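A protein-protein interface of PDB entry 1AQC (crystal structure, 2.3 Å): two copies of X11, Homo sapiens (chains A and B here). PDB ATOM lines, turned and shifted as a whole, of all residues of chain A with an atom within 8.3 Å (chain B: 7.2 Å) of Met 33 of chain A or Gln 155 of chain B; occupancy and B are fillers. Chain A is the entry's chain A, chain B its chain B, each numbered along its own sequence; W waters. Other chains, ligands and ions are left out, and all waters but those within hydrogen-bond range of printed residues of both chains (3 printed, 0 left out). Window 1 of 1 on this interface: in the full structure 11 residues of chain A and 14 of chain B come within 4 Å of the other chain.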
ATOM      1  N   LEU A  20      23.928   9.356 -17.739  1.00  0.00           N
ATOM      2  CA  LEU A  20      25.208   8.690 -17.587  1.00  0.00           C
ATOM      3  C   LEU A  20      25.845   8.429 -18.937  1.00  0.00           C
ATOM      4  O   LEU A  20      25.211   8.601 -19.985  1.00  0.00           O
ATOM      5  CB  LEU A  20      25.024   7.338 -16.849  1.00  0.00           C
ATOM      6  CG  LEU A  20      24.157   6.199 -17.429  1.00  0.00           C
ATOM      7  CD1 LEU A  20      24.634   4.865 -16.917  1.00  0.00           C
ATOM      8  CD2 LEU A  20      22.672   6.395 -17.117  1.00  0.00           C
ATOM      9  N   SER A  27      28.310  -5.158 -19.681  1.00  0.00           N
ATOM     10  CA  SER A  27      27.985  -6.421 -19.079  1.00  0.00           C
ATOM     11  C   SER A  27      26.844  -6.113 -18.112  1.00  0.00           C
ATOM     12  O   SER A  27      26.670  -4.971 -17.673  1.00  0.00           O
ATOM     13  CB  SER A  27      29.203  -7.013 -18.354  1.00  0.00           C
ATOM     14  OG  SER A  27      29.576  -6.260 -17.209  1.00  0.00           O
ATOM     15  N   LYS A  28      26.072  -7.144 -17.789  1.00  0.00           N
ATOM     16  CA  LYS A  28      24.937  -7.037 -16.887  1.00  0.00           C
ATOM     17  C   LYS A  28      25.260  -6.444 -15.507  1.00  0.00           C
ATOM     18  O   LYS A  28      24.505  -5.624 -14.987  1.00  0.00           O
ATOM     19  CB  LYS A  28      24.254  -8.402 -16.742  1.00  0.00           C
ATOM     20  CG  LYS A  28      24.842  -9.316 -15.672  1.00  0.00           C
ATOM     21  CD  LYS A  28      23.769 -10.292 -15.170  1.00  0.00           C
ATOM     22  CE  LYS A  28      24.057 -10.760 -13.748  1.00  0.00           C
ATOM     23  NZ  LYS A  28      24.130  -9.617 -12.781  1.00  0.00           N
ATOM     24  N   ASN A  29      26.389  -6.832 -14.927  1.00  0.00           N
ATOM     25  CA  ASN A  29      26.774  -6.325 -13.619  1.00  0.00           C
ATOM     26  C   ASN A  29      27.069  -4.848 -13.620  1.00  0.00           C
ATOM     27  O   ASN A  29      26.760  -4.144 -12.663  1.00  0.00           O
ATOM     28  CB  ASN A  29      27.969  -7.083 -13.116  1.00  0.00           C
ATOM     29  CG  ASN A  29      27.709  -8.535 -13.082  1.00  0.00           C
ATOM     30  OD1 ASN A  29      27.933  -9.250 -14.077  1.00  0.00           O
ATOM     31  ND2 ASN A  29      27.120  -8.988 -11.988  1.00  0.00           N
ATOM     32  N   VAL A  30      27.691  -4.378 -14.691  1.00  0.00           N
ATOM     33  CA  VAL A  30      28.009  -2.968 -14.811  1.00  0.00           C
ATOM     34  C   VAL A  30      26.693  -2.224 -15.074  1.00  0.00           C
ATOM     35  O   VAL A  30      26.469  -1.118 -14.560  1.00  0.00           O
ATOM     36  CB  VAL A  30      29.037  -2.750 -15.918  1.00  0.00           C
ATOM     37  CG1 VAL A  30      29.368  -1.277 -16.045  1.00  0.00           C
ATOM     38  CG2 VAL A  30      30.293  -3.550 -15.607  1.00  0.00           C
ATOM     39  N   ARG A  31      25.795  -2.881 -15.803  1.00  0.00           N
ATOM     40  CA  ARG A  31      24.487  -2.317 -16.102  1.00  0.00           C
ATOM     41  C   ARG A  31      23.598  -2.245 -14.843  1.00  0.00           C
ATOM     42  O   ARG A  31      22.646  -1.471 -14.788  1.00  0.00           O
ATOM     43  CB  ARG A  31      23.810  -3.122 -17.207  1.00  0.00           C
ATOM     44  CG  ARG A  31      22.703  -2.371 -17.912  1.00  0.00           C
ATOM     45  CD  ARG A  31      22.975  -2.179 -19.373  1.00  0.00           C
ATOM     46  NE  ARG A  31      23.084  -0.768 -19.712  1.00  0.00           N
ATOM     47  CZ  ARG A  31      23.145  -0.295 -20.957  1.00  0.00           C
ATOM     48  NH1 ARG A  31      23.096  -1.124 -21.991  1.00  0.00           N
ATOM     49  NH2 ARG A  31      23.299   1.011 -21.172  1.00  0.00           N
ATOM     50  N   MET A  32      23.881  -3.077 -13.845  1.00  0.00           N
ATOM     51  CA  MET A  32      23.128  -3.043 -12.593  1.00  0.00           C
ATOM     52  C   MET A  32      23.659  -1.894 -11.764  1.00  0.00           C
ATOM     53  O   MET A  32      22.884  -1.218 -11.095  1.00  0.00           O
ATOM     54  CB  MET A  32      23.246  -4.348 -11.820  1.00  0.00           C
ATOM     55  CG  MET A  32      22.118  -5.357 -12.083  1.00  0.00           C
ATOM     56  SD  MET A  32      20.437  -4.869 -11.495  1.00  0.00           S
ATOM     57  CE  MET A  32      20.807  -4.225  -9.812  1.00  0.00           C
ATOM     58  N   MET A  33      24.975  -1.657 -11.841  1.00  0.00           N
ATOM     59  CA  MET A  33      25.645  -0.546 -11.132  1.00  0.00           C
ATOM     60  C   MET A  33      25.125   0.815 -11.650  1.00  0.00           C
ATOM     61  O   MET A  33      25.134   1.826 -10.951  1.00  0.00           O
ATOM     62  CB  MET A  33      27.177  -0.621 -11.310  1.00  0.00           C
ATOM     63  CG  MET A  33      27.918  -1.588 -10.362  1.00  0.00           C
ATOM     64  SD  MET A  33      29.759  -1.441 -10.322  1.00  0.00           S
ATOM     65  CE  MET A  33      29.992  -0.155  -9.086  1.00  0.00           C
ATOM     66  N   GLN A  34      24.683   0.829 -12.902  1.00  0.00           N
ATOM     67  CA  GLN A  34      24.128   2.025 -13.522  1.00  0.00           C
ATOM     68  C   GLN A  34      22.750   2.323 -12.940  1.00  0.00           C
ATOM     69  O   GLN A  34      22.458   3.448 -12.520  1.00  0.00           O
ATOM     70  CB  GLN A  34      24.022   1.793 -15.007  1.00  0.00           C
ATOM     71  CG  GLN A  34      25.318   1.389 -15.583  1.00  0.00           C
ATOM     72  CD  GLN A  34      25.264   1.368 -17.054  1.00  0.00           C
ATOM     73  OE1 GLN A  34      24.245   1.002 -17.641  1.00  0.00           O
ATOM     74  NE2 GLN A  34      26.349   1.778 -17.684  1.00  0.00           N
ATOM     75  N   ALA A  35      21.910   1.295 -12.927  1.00  0.00           N
ATOM     76  CA  ALA A  35      20.572   1.381 -12.374  1.00  0.00           C
ATOM     77  C   ALA A  35      20.691   1.842 -10.910  1.00  0.00           C
ATOM     78  O   ALA A  35      20.137   2.869 -10.526  1.00  0.00           O
ATOM     79  CB  ALA A  35      19.901   0.007 -12.458  1.00  0.00           C
ATOM     80  N   GLN A  36      21.470   1.099 -10.129  1.00  0.00           N
ATOM     81  CA  GLN A  36      21.715   1.383  -8.727  1.00  0.00           C
ATOM     82  C   GLN A  36      22.206   2.797  -8.535  1.00  0.00           C
ATOM     83  O   GLN A  36      21.977   3.410  -7.495  1.00  0.00           O
ATOM     84  CB  GLN A  36      22.777   0.431  -8.176  1.00  0.00           C
ATOM     85  CG  GLN A  36      22.433  -1.029  -8.301  1.00  0.00           C
ATOM     86  CD  GLN A  36      23.561  -1.922  -7.841  1.00  0.00           C
ATOM     87  OE1 GLN A  36      24.729  -1.692  -8.161  1.00  0.00           O
ATOM     88  NE2 GLN A  36      23.217  -2.959  -7.101  1.00  0.00           N
ATOM     89  N   GLU A  37      22.902   3.307  -9.537  1.00  0.00           N
ATOM     90  CA  GLU A  37      23.415   4.657  -9.474  1.00  0.00           C
ATOM     91  C   GLU A  37      22.271   5.652  -9.608  1.00  0.00           C
ATOM     92  O   GLU A  37      22.130   6.544  -8.760  1.00  0.00           O
ATOM     93  CB  GLU A  37      24.471   4.882 -10.554  1.00  0.00           C
ATOM     94  CG  GLU A  37      25.234   6.179 -10.376  1.00  0.00           C
ATOM     95  CD  GLU A  37      26.542   6.209 -11.143  1.00  0.00           C
ATOM     96  OE1 GLU A  37      26.511   6.451 -12.371  1.00  0.00           O
ATOM     97  OE2 GLU A  37      27.604   6.003 -10.510  1.00  0.00           O
ATOM     98  N   ALA A  38      21.429   5.467 -10.631  1.00  0.00           N
ATOM     99  CA  ALA A  38      20.271   6.343 -10.873  1.00  0.00           C
ATOM    100  C   ALA A  38      19.427   6.435  -9.603  1.00  0.00           C
ATOM    101  O   ALA A  38      19.017   7.515  -9.203  1.00  0.00           O
ATOM    102  CB  ALA A  38      19.432   5.800 -12.006  1.00  0.00           C
ATOM    103  N   VAL A  39      19.209   5.284  -8.967  1.00  0.00           N
ATOM    104  CA  VAL A  39      18.434   5.164  -7.735  1.00  0.00           C
ATOM    105  C   VAL A  39      19.094   5.953  -6.616  1.00  0.00           C
ATOM    106  O   VAL A  39      18.418   6.524  -5.763  1.00  0.00           O
ATOM    107  CB  VAL A  39      18.325   3.679  -7.273  1.00  0.00           C
ATOM    108  CG1 VAL A  39      17.587   3.585  -5.937  1.00  0.00           C
ATOM    109  CG2 VAL A  39      17.639   2.834  -8.335  1.00  0.00           C
ATOM    110  N   SER A  40      20.420   5.961  -6.612  1.00  0.00           N
ATOM    111  CA  SER A  40      21.192   6.667  -5.592  1.00  0.00           C
ATOM    112  C   SER A  40      21.013   8.152  -5.736  1.00  0.00           C
ATOM    113  O   SER A  40      20.704   8.842  -4.776  1.00  0.00           O
ATOM    114  CB  SER A  40      22.678   6.337  -5.713  1.00  0.00           C
ATOM    115  OG  SER A  40      22.938   5.013  -5.295  1.00  0.00           O
ATOM    116  N   TYR A  96      17.889  -0.944 -21.385  1.00  0.00           N
ATOM    117  CA  TYR A  96      17.865  -1.821 -20.214  1.00  0.00           C
ATOM    118  C   TYR A  96      16.740  -1.372 -19.272  1.00  0.00           C
ATOM    119  O   TYR A  96      16.288  -0.230 -19.338  1.00  0.00           O
ATOM    120  CB  TYR A  96      19.237  -1.727 -19.508  1.00  0.00           C
ATOM    121  CG  TYR A  96      19.392  -2.499 -18.216  1.00  0.00           C
ATOM    122  CD1 TYR A  96      19.768  -3.828 -18.225  1.00  0.00           C
ATOM    123  CD2 TYR A  96      19.239  -1.867 -16.972  1.00  0.00           C
ATOM    124  CE1 TYR A  96      20.000  -4.523 -17.030  1.00  0.00           C
ATOM    125  CE2 TYR A  96      19.470  -2.550 -15.762  1.00  0.00           C
ATOM    126  CZ  TYR A  96      19.852  -3.875 -15.810  1.00  0.00           C
ATOM    127  OH  TYR A  96      20.103  -4.565 -14.662  1.00  0.00           O
ATOM    128  N   ALA A  98      15.354  -2.333 -15.078  1.00  0.00           N
ATOM    129  CA  ALA A  98      15.604  -3.114 -13.882  1.00  0.00           C
ATOM    130  C   ALA A  98      14.663  -2.743 -12.764  1.00  0.00           C
ATOM    131  O   ALA A  98      14.192  -1.618 -12.697  1.00  0.00           O
ATOM    132  CB  ALA A  98      17.061  -2.922 -13.427  1.00  0.00           C
ATOM    133  N   ILE A 100      14.633  -2.567  -8.763  1.00  0.00           N
ATOM    134  CA  ILE A 100      15.507  -2.584  -7.584  1.00  0.00           C
ATOM    135  C   ILE A 100      14.543  -2.407  -6.436  1.00  0.00           C
ATOM    136  O   ILE A 100      14.148  -1.287  -6.098  1.00  0.00           O
ATOM    137  CB  ILE A 100      16.595  -1.433  -7.566  1.00  0.00           C
ATOM    138  CG1 ILE A 100      17.688  -1.648  -8.633  1.00  0.00           C
ATOM    139  CG2 ILE A 100      17.305  -1.425  -6.206  1.00  0.00           C
ATOM    140  CD1 ILE A 100      17.365  -1.134  -9.984  1.00  0.00           C
ATOM    141  N   MET A 107      16.281   2.833 -18.658  1.00  0.00           N
ATOM    142  CA  MET A 107      17.362   3.554 -19.318  1.00  0.00           C
ATOM    143  C   MET A 107      17.140   3.601 -20.839  1.00  0.00           C
ATOM    144  O   MET A 107      16.838   2.577 -21.475  1.00  0.00           O
ATOM    145  CB  MET A 107      18.692   2.896 -18.972  1.00  0.00           C
ATOM    146  CG  MET A 107      19.930   3.625 -19.489  1.00  0.00           C
ATOM    147  SD  MET A 107      21.393   2.554 -19.400  1.00  0.00           S
ATOM    148  CE  MET A 107      21.104   1.831 -17.752  1.00  0.00           C
ATOM    149  N   ILE B   8      27.740   6.319  -7.224  1.00  0.00           N
ATOM    150  CA  ILE B   8      26.725   5.788  -6.277  1.00  0.00           C
ATOM    151  C   ILE B   8      27.117   6.226  -4.865  1.00  0.00           C
ATOM    152  O   ILE B   8      28.215   5.922  -4.399  1.00  0.00           O
ATOM    153  CB  ILE B   8      26.673   4.263  -6.318  1.00  0.00           C
ATOM    154  CG1 ILE B   8      26.470   3.771  -7.755  1.00  0.00           C
ATOM    155  CG2 ILE B   8      25.577   3.766  -5.418  1.00  0.00           C
ATOM    156  CD1 ILE B   8      26.793   2.275  -7.954  1.00  0.00           C
ATOM    157  N   ILE B  70      30.270   4.458  -3.188  1.00  0.00           N
ATOM    158  CA  ILE B  70      30.611   3.109  -3.636  1.00  0.00           C
ATOM    159  C   ILE B  70      31.126   3.234  -5.055  1.00  0.00           C
ATOM    160  O   ILE B  70      30.498   3.923  -5.869  1.00  0.00           O
ATOM    161  CB  ILE B  70      29.377   2.174  -3.666  1.00  0.00           C
ATOM    162  CG1 ILE B  70      28.865   1.888  -2.253  1.00  0.00           C
ATOM    163  CG2 ILE B  70      29.716   0.890  -4.406  1.00  0.00           C
ATOM    164  CD1 ILE B  70      27.460   1.327  -2.233  1.00  0.00           C
ATOM    165  N   LEU B  71      32.214   2.517  -5.355  1.00  0.00           N
ATOM    166  CA  LEU B  71      32.863   2.534  -6.677  1.00  0.00           C
ATOM    167  C   LEU B  71      33.605   1.207  -6.912  1.00  0.00           C
ATOM    168  O   LEU B  71      33.827   0.437  -5.971  1.00  0.00           O
ATOM    169  CB  LEU B  71      33.878   3.684  -6.732  1.00  0.00           C
ATOM    170  CG  LEU B  71      34.402   4.246  -8.053  1.00  0.00           C
ATOM    171  CD1 LEU B  71      33.281   4.987  -8.790  1.00  0.00           C
ATOM    172  CD2 LEU B  71      35.582   5.197  -7.772  1.00  0.00           C
ATOM    173  N   THR B  72      33.982   0.939  -8.162  1.00  0.00           N
ATOM    174  CA  THR B  72      34.715  -0.274  -8.468  1.00  0.00           C
ATOM    175  C   THR B  72      36.114  -0.137  -7.899  1.00  0.00           C
ATOM    176  O   THR B  72      36.746  -1.117  -7.544  1.00  0.00           O
ATOM    177  CB  THR B  72      34.856  -0.556 -10.005  1.00  0.00           C
ATOM    178  OG1 THR B  72      35.369   0.593 -10.680  1.00  0.00           O
ATOM    179  CG2 THR B  72      33.541  -0.953 -10.623  1.00  0.00           C
ATOM    180  N   GLN B  73      36.608   1.088  -7.826  1.00  0.00           N
ATOM    181  CA  GLN B  73      37.948   1.320  -7.327  1.00  0.00           C
ATOM    182  C   GLN B  73      38.020   1.278  -5.797  1.00  0.00           C
ATOM    183  O   GLN B  73      38.916   0.655  -5.222  1.00  0.00           O
ATOM    184  CB  GLN B  73      38.469   2.658  -7.858  1.00  0.00           C
ATOM    185  CG  GLN B  73      38.197   2.948  -9.366  1.00  0.00           C
ATOM    186  CD  GLN B  73      38.951   2.033 -10.348  1.00  0.00           C
ATOM    187  OE1 GLN B  73      38.338   1.329 -11.166  1.00  0.00           O
ATOM    188  NE2 GLN B  73      40.278   2.065 -10.289  1.00  0.00           N
ATOM    189  N   LEU B  91      38.866  -1.013  -2.660  1.00  0.00           N
ATOM    190  CA  LEU B  91      38.031  -2.203  -2.858  1.00  0.00           C
ATOM    191  C   LEU B  91      38.735  -3.545  -2.663  1.00  0.00           C
ATOM    192  O   LEU B  91      38.188  -4.434  -2.020  1.00  0.00           O
ATOM    193  CB  LEU B  91      37.351  -2.149  -4.240  1.00  0.00           C
ATOM    194  CG  LEU B  91      35.855  -2.479  -4.449  1.00  0.00           C
ATOM    195  CD1 LEU B  91      35.637  -3.885  -4.942  1.00  0.00           C
ATOM    196  CD2 LEU B  91      35.071  -2.216  -3.185  1.00  0.00           C
ATOM    197  N   ILE B 149      22.580  -0.940  -0.128  1.00  0.00           N
ATOM    198  CA  ILE B 149      23.988  -0.634   0.018  1.00  0.00           C
ATOM    199  C   ILE B 149      24.838  -1.904  -0.166  1.00  0.00           C
ATOM    200  O   ILE B 149      25.772  -1.913  -0.980  1.00  0.00           O
ATOM    201  CB  ILE B 149      24.278   0.074   1.384  1.00  0.00           C
ATOM    202  CG1 ILE B 149      23.690   1.497   1.373  1.00  0.00           C
ATOM    203  CG2 ILE B 149      25.776   0.149   1.653  1.00  0.00           C
ATOM    204  CD1 ILE B 149      23.907   2.278   2.651  1.00  0.00           C
ATOM    205  N   ALA B 150      24.490  -2.985   0.527  1.00  0.00           N
ATOM    206  CA  ALA B 150      25.234  -4.227   0.393  1.00  0.00           C
ATOM    207  C   ALA B 150      25.158  -4.777  -1.047  1.00  0.00           C
ATOM    208  O   ALA B 150      26.183  -5.216  -1.601  1.00  0.00           O
ATOM    209  CB  ALA B 150      24.740  -5.247   1.388  1.00  0.00           C
ATOM    210  N   GLN B 151      23.974  -4.706  -1.673  1.00  0.00           N
ATOM    211  CA  GLN B 151      23.777  -5.196  -3.047  1.00  0.00           C
ATOM    212  C   GLN B 151      24.682  -4.411  -3.983  1.00  0.00           C
ATOM    213  O   GLN B 151      25.311  -4.986  -4.871  1.00  0.00           O
ATOM    214  CB  GLN B 151      22.318  -5.042  -3.506  1.00  0.00           C
ATOM    215  CG  GLN B 151      21.320  -6.047  -2.925  1.00  0.00           C
ATOM    216  CD  GLN B 151      19.856  -5.616  -3.116  1.00  0.00           C
ATOM    217  OE1 GLN B 151      19.565  -4.579  -3.702  1.00  0.00           O
ATOM    218  NE2 GLN B 151      18.940  -6.403  -2.603  1.00  0.00           N
ATOM    219  N   SER B 152      24.792  -3.107  -3.744  1.00  0.00           N
ATOM    220  CA  SER B 152      25.629  -2.238  -4.567  1.00  0.00           C
ATOM    221  C   SER B 152      27.115  -2.534  -4.410  1.00  0.00           C
ATOM    222  O   SER B 152      27.873  -2.499  -5.390  1.00  0.00           O
ATOM    223  CB  SER B 152      25.360  -0.769  -4.248  1.00  0.00           C
ATOM    224  OG  SER B 152      24.027  -0.431  -4.570  1.00  0.00           O
ATOM    225  N   ILE B 153      27.553  -2.819  -3.190  1.00  0.00           N
ATOM    226  CA  ILE B 153      28.967  -3.112  -3.001  1.00  0.00           C
ATOM    227  C   ILE B 153      29.258  -4.439  -3.687  1.00  0.00           C
ATOM    228  O   ILE B 153      30.285  -4.598  -4.341  1.00  0.00           O
ATOM    229  CB  ILE B 153      29.369  -3.147  -1.503  1.00  0.00           C
ATOM    230  CG1 ILE B 153      29.182  -1.765  -0.873  1.00  0.00           C
ATOM    231  CG2 ILE B 153      30.812  -3.577  -1.347  1.00  0.00           C
ATOM    232  CD1 ILE B 153      29.695  -1.668   0.538  1.00  0.00           C
ATOM    233  N   GLY B 154      28.308  -5.363  -3.604  1.00  0.00           N
ATOM    234  CA  GLY B 154      28.486  -6.650  -4.234  1.00  0.00           C
ATOM    235  C   GLY B 154      28.653  -6.525  -5.732  1.00  0.00           C
ATOM    236  O   GLY B 154      29.370  -7.325  -6.340  1.00  0.00           O
ATOM    237  N   GLN B 155      27.963  -5.554  -6.333  1.00  0.00           N
ATOM    238  CA  GLN B 155      28.055  -5.332  -7.779  1.00  0.00           C
ATOM    239  C   GLN B 155      29.431  -4.772  -8.085  1.00  0.00           C
ATOM    240  O   GLN B 155      30.082  -5.172  -9.061  1.00  0.00           O
ATOM    241  CB  GLN B 155      26.945  -4.393  -8.291  1.00  0.00           C
ATOM    242  CG  GLN B 155      25.536  -5.021  -8.377  1.00  0.00           C
ATOM    243  CD  GLN B 155      25.444  -6.264  -9.287  1.00  0.00           C
ATOM    244  OE1 GLN B 155      26.341  -6.539 -10.098  1.00  0.00           O
ATOM    245  NE2 GLN B 155      24.353  -7.018  -9.148  1.00  0.00           N
ATOM    246  N   ALA B 156      29.893  -3.879  -7.214  1.00  0.00           N
ATOM    247  CA  ALA B 156      31.223  -3.295  -7.347  1.00  0.00           C
ATOM    248  C   ALA B 156      32.240  -4.449  -7.347  1.00  0.00           C
ATOM    249  O   ALA B 156      33.161  -4.496  -8.155  1.00  0.00           O
ATOM    250  CB  ALA B 156      31.487  -2.339  -6.183  1.00  0.00           C
ATOM    251  N   PHE B 157      32.027  -5.412  -6.457  1.00  0.00           N
ATOM    252  CA  PHE B 157      32.891  -6.588  -6.337  1.00  0.00           C
ATOM    253  C   PHE B 157      32.948  -7.351  -7.652  1.00  0.00           C
ATOM    254  O   PHE B 157      34.028  -7.706  -8.145  1.00  0.00           O
ATOM    255  CB  PHE B 157      32.359  -7.523  -5.233  1.00  0.00           C
ATOM    256  CG  PHE B 157      32.619  -7.031  -3.837  1.00  0.00           C
ATOM    257  CD1 PHE B 157      33.456  -5.955  -3.607  1.00  0.00           C
ATOM    258  CD2 PHE B 157      32.062  -7.674  -2.745  1.00  0.00           C
ATOM    259  CE1 PHE B 157      33.728  -5.538  -2.328  1.00  0.00           C
ATOM    260  CE2 PHE B 157      32.340  -7.250  -1.455  1.00  0.00           C
ATOM    261  CZ  PHE B 157      33.170  -6.186  -1.254  1.00  0.00           C
ATOM    262  N   SER B 158      31.757  -7.572  -8.204  1.00  0.00           N
ATOM    263  CA  SER B 158      31.545  -8.302  -9.445  1.00  0.00           C
ATOM    264  C   SER B 158      32.230  -7.650 -10.614  1.00  0.00           C
ATOM    265  O   SER B 158      32.867  -8.336 -11.413  1.00  0.00           O
ATOM    266  CB  SER B 158      30.051  -8.429  -9.713  1.00  0.00           C
ATOM    267  OG  SER B 158      29.382  -8.944  -8.559  1.00  0.00           O
ATOM    268  N   VAL B 159      32.111  -6.327 -10.700  1.00  0.00           N
ATOM    269  CA  VAL B 159      32.736  -5.552 -11.782  1.00  0.00           C
ATOM    270  C   VAL B 159      34.253  -5.484 -11.641  1.00  0.00           C
ATOM    271  O   VAL B 159      34.980  -5.746 -12.587  1.00  0.00           O
ATOM    272  CB  VAL B 159      32.189  -4.109 -11.849  1.00  0.00           C
ATOM    273  CG1 VAL B 159      32.908  -3.321 -12.927  1.00  0.00           C
ATOM    274  CG2 VAL B 159      30.705  -4.127 -12.109  1.00  0.00           C
ATOM    275  N   ALA B 160      34.725  -5.102 -10.462  1.00  0.00           N
ATOM    276  CA  ALA B 160      36.158  -5.007 -10.212  1.00  0.00           C
ATOM    277  C   ALA B 160      36.850  -6.384 -10.362  1.00  0.00           C
ATOM    278  O   ALA B 160      38.010  -6.476 -10.774  1.00  0.00           O
ATOM    279  CB  ALA B 160      36.408  -4.400  -8.826  1.00  0.00           C
ATOM    280  N   TYR B 161      36.114  -7.455 -10.093  1.00  0.00           N
ATOM    281  CA  TYR B 161      36.671  -8.799 -10.207  1.00  0.00           C
ATOM    282  C   TYR B 161      36.843  -9.117 -11.680  1.00  0.00           C
ATOM    283  O   TYR B 161      37.799  -9.777 -12.074  1.00  0.00           O
ATOM    284  CB  TYR B 161      35.751  -9.817  -9.524  1.00  0.00           C
ATOM    285  CG  TYR B 161      36.184 -11.265  -9.639  1.00  0.00           C
ATOM    286  CD1 TYR B 161      37.460 -11.672  -9.257  1.00  0.00           C
ATOM    287  CD2 TYR B 161      35.298 -12.236 -10.120  1.00  0.00           C
ATOM    288  CE1 TYR B 161      37.845 -13.019  -9.354  1.00  0.00           C
ATOM    289  CE2 TYR B 161      35.671 -13.570 -10.216  1.00  0.00           C
ATOM    290  CZ  TYR B 161      36.942 -13.953  -9.831  1.00  0.00           C
ATOM    291  OH  TYR B 161      37.287 -15.275  -9.906  1.00  0.00           O
ATOM    292  N   GLN B 162      35.912  -8.624 -12.489  1.00  0.00           N
ATOM    293  CA  GLN B 162      35.956  -8.844 -13.922  1.00  0.00           C
ATOM    294  C   GLN B 162      37.183  -8.139 -14.428  1.00  0.00           C
ATOM    295  O   GLN B 162      37.928  -8.670 -15.248  1.00  0.00           O
ATOM    296  CB  GLN B 162      34.721  -8.244 -14.603  1.00  0.00           C
ATOM    297  CG  GLN B 162      33.473  -9.087 -14.539  1.00  0.00           C
ATOM    298  CD  GLN B 162      32.240  -8.341 -15.016  1.00  0.00           C
ATOM    299  OE1 GLN B 162      32.324  -7.245 -15.580  1.00  0.00           O
ATOM    300  NE2 GLN B 162      31.087  -8.929 -14.780  1.00  0.00           N
HETATM  301  O   HOH W   1      20.282  -3.670  -6.073  1.00  0.00           O
HETATM  302  O   HOH W   2      29.152   8.418  -9.273  1.00  0.00           O
HETATM  303  O   HOH W   3      22.452  -8.263 -11.454  1.00  0.00           O
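ND2 of Asn 29 of chain A touches CB of Ser 158 of chain B (3.8 Å).
Asn 29 of chain A touches Val 159 of chain B (O to CG2, 3.98 Å).
CG2 of Val 159 of chain B touches CG2 of Val 30 of chain A (3.6 Å).
Met 32 of chain A touches Gln 155 of chain B.
Met 33 of chain A touches Ile 8 of chain B (O to CD1, 3.5 Å).
Met 33 of chain A touches Thr 72 of chain B.
Val 159 of chain B touches Met 33 of chain A.
Gln 151 of chain B touches Gln 36 of chain A (O to NE2, 3.7 Å).
Gln 155 of chain B touches Gln 36 of chain A (CG to NE2, 3.4 Å).
Ile 8 of chain B touches Ser 40 of chain A (CG2 to OG, 2.9 Å).
The side-chain amino group (NZ) of Lys 28 of chain A lies close to the side-chain amide nitrogen (ND2) of Asn 29 of chain A, at 3.2 Å.
The backbone carbonyl oxygen (O) of Met 32 of chain A lies close to the side-chain amide oxygen (OE1) of Gln 36 of chain A (3.5 Å).
The side-chain sulfur of Met 32 of chain A is in hydrogen-bond range of the side-chain hydroxyl of Tyr 96 of chain A, 3.2 Å away.
The backbone NH (N) of Ile 70 of chain B lies within hydrogen-bond range of the backbone carbonyl oxygen (O) of Ile 8 of chain B, at 2.8 Å.
The side-chain amide oxygen of Gln 73 of chain B sits at hydrogen-bond distance from the side-chain hydroxyl of Thr 72 of chain B (3.1 Å).
O of Gly 154 of chain B is in hydrogen-bond range of OG of Ser 158 of chain B (2.7 Å).
OG of Ser 27 of chain A sits at hydrogen-bond distance from OE1 of Gln 162 of chain B (3.3 Å).
The side-chain amide oxygen (OE1) of Gln 155 of chain B sits at hydrogen-bond distance from the side-chain amide nitrogen (ND2) of Asn 29 of chain A (3.2 Å).
The side-chain amide oxygen (OD1) of Asn 29 of chain A lies within hydrogen-bond range of the side-chain amide nitrogen (NE2) of Gln 162 of chain B, at 3.2 Å.
N of Ile 8 of chain B sits at hydrogen-bond distance from OE2 of Glu 37 of chain A, 3.3 Å away.
Met 33 of chain A touches five residues of chain B.
Of the printed residues of chain A, Thr 72 of chain B touches Met 33.
Of the printed residues of chain A, Gln 155 of chain B touches Asn 29, Met 32, Met 33 and Gln 36.
Printed residues of chain A within 4 Å of Ser 158 of chain B: Asn 29.
The nearest residue of chain B that does not touch Met 33 of chain A is Leu 71 of chain B (4.4 Å).
The nearest printed residue of chain A that does not touch Ile 8 of chain B is Gln 36 of chain A (4.2 Å).
Water W3 lies within hydrogen-bond range of NZ of Lys 28 of chain A (2.5 Å) and NE2 of Gln 155 of chain B (3.2 Å).
Water W1 bridges OE1 of Gln 151 of chain B (2.6 Å) and NE2 of Gln 36 of chain A (3.2 Å).
Water W2 lies within hydrogen-bond range of OE2 of Glu 37 of chain A (3.1 Å) and N of Ile 8 of chain B (3.3 Å).
Of the 19 printed residues of chain A, 8 touch a printed residue of chain B.
Hydrophobic or aromatic side chains of chain A that line the printed part of chain B: Val 30, Met 32 and Met 33.
Printed residues of chain B that touch a printed residue of chain A: Ile 8, Thr 72, Gln 151, Ser 152, Gln 155, Ala 156, Ser 158, Val 159 and Gln 162.
Hydrophobic or aromatic side chains of chain B within 4 Å of the printed part of chain A: Ile 8, Ala 156 and Val 159.
Among the printed residues, 17 pairs touch across the chains.
Among the printed residues, no Asp or Glu carboxylate lies within 4 Å of a Lys or Arg side-chain nitrogen of the other chain.
No position is printed for both chains.
Of the 17 pairs that touch across the chains among the printed residues, none has its exchanged pair printed and touching as well.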
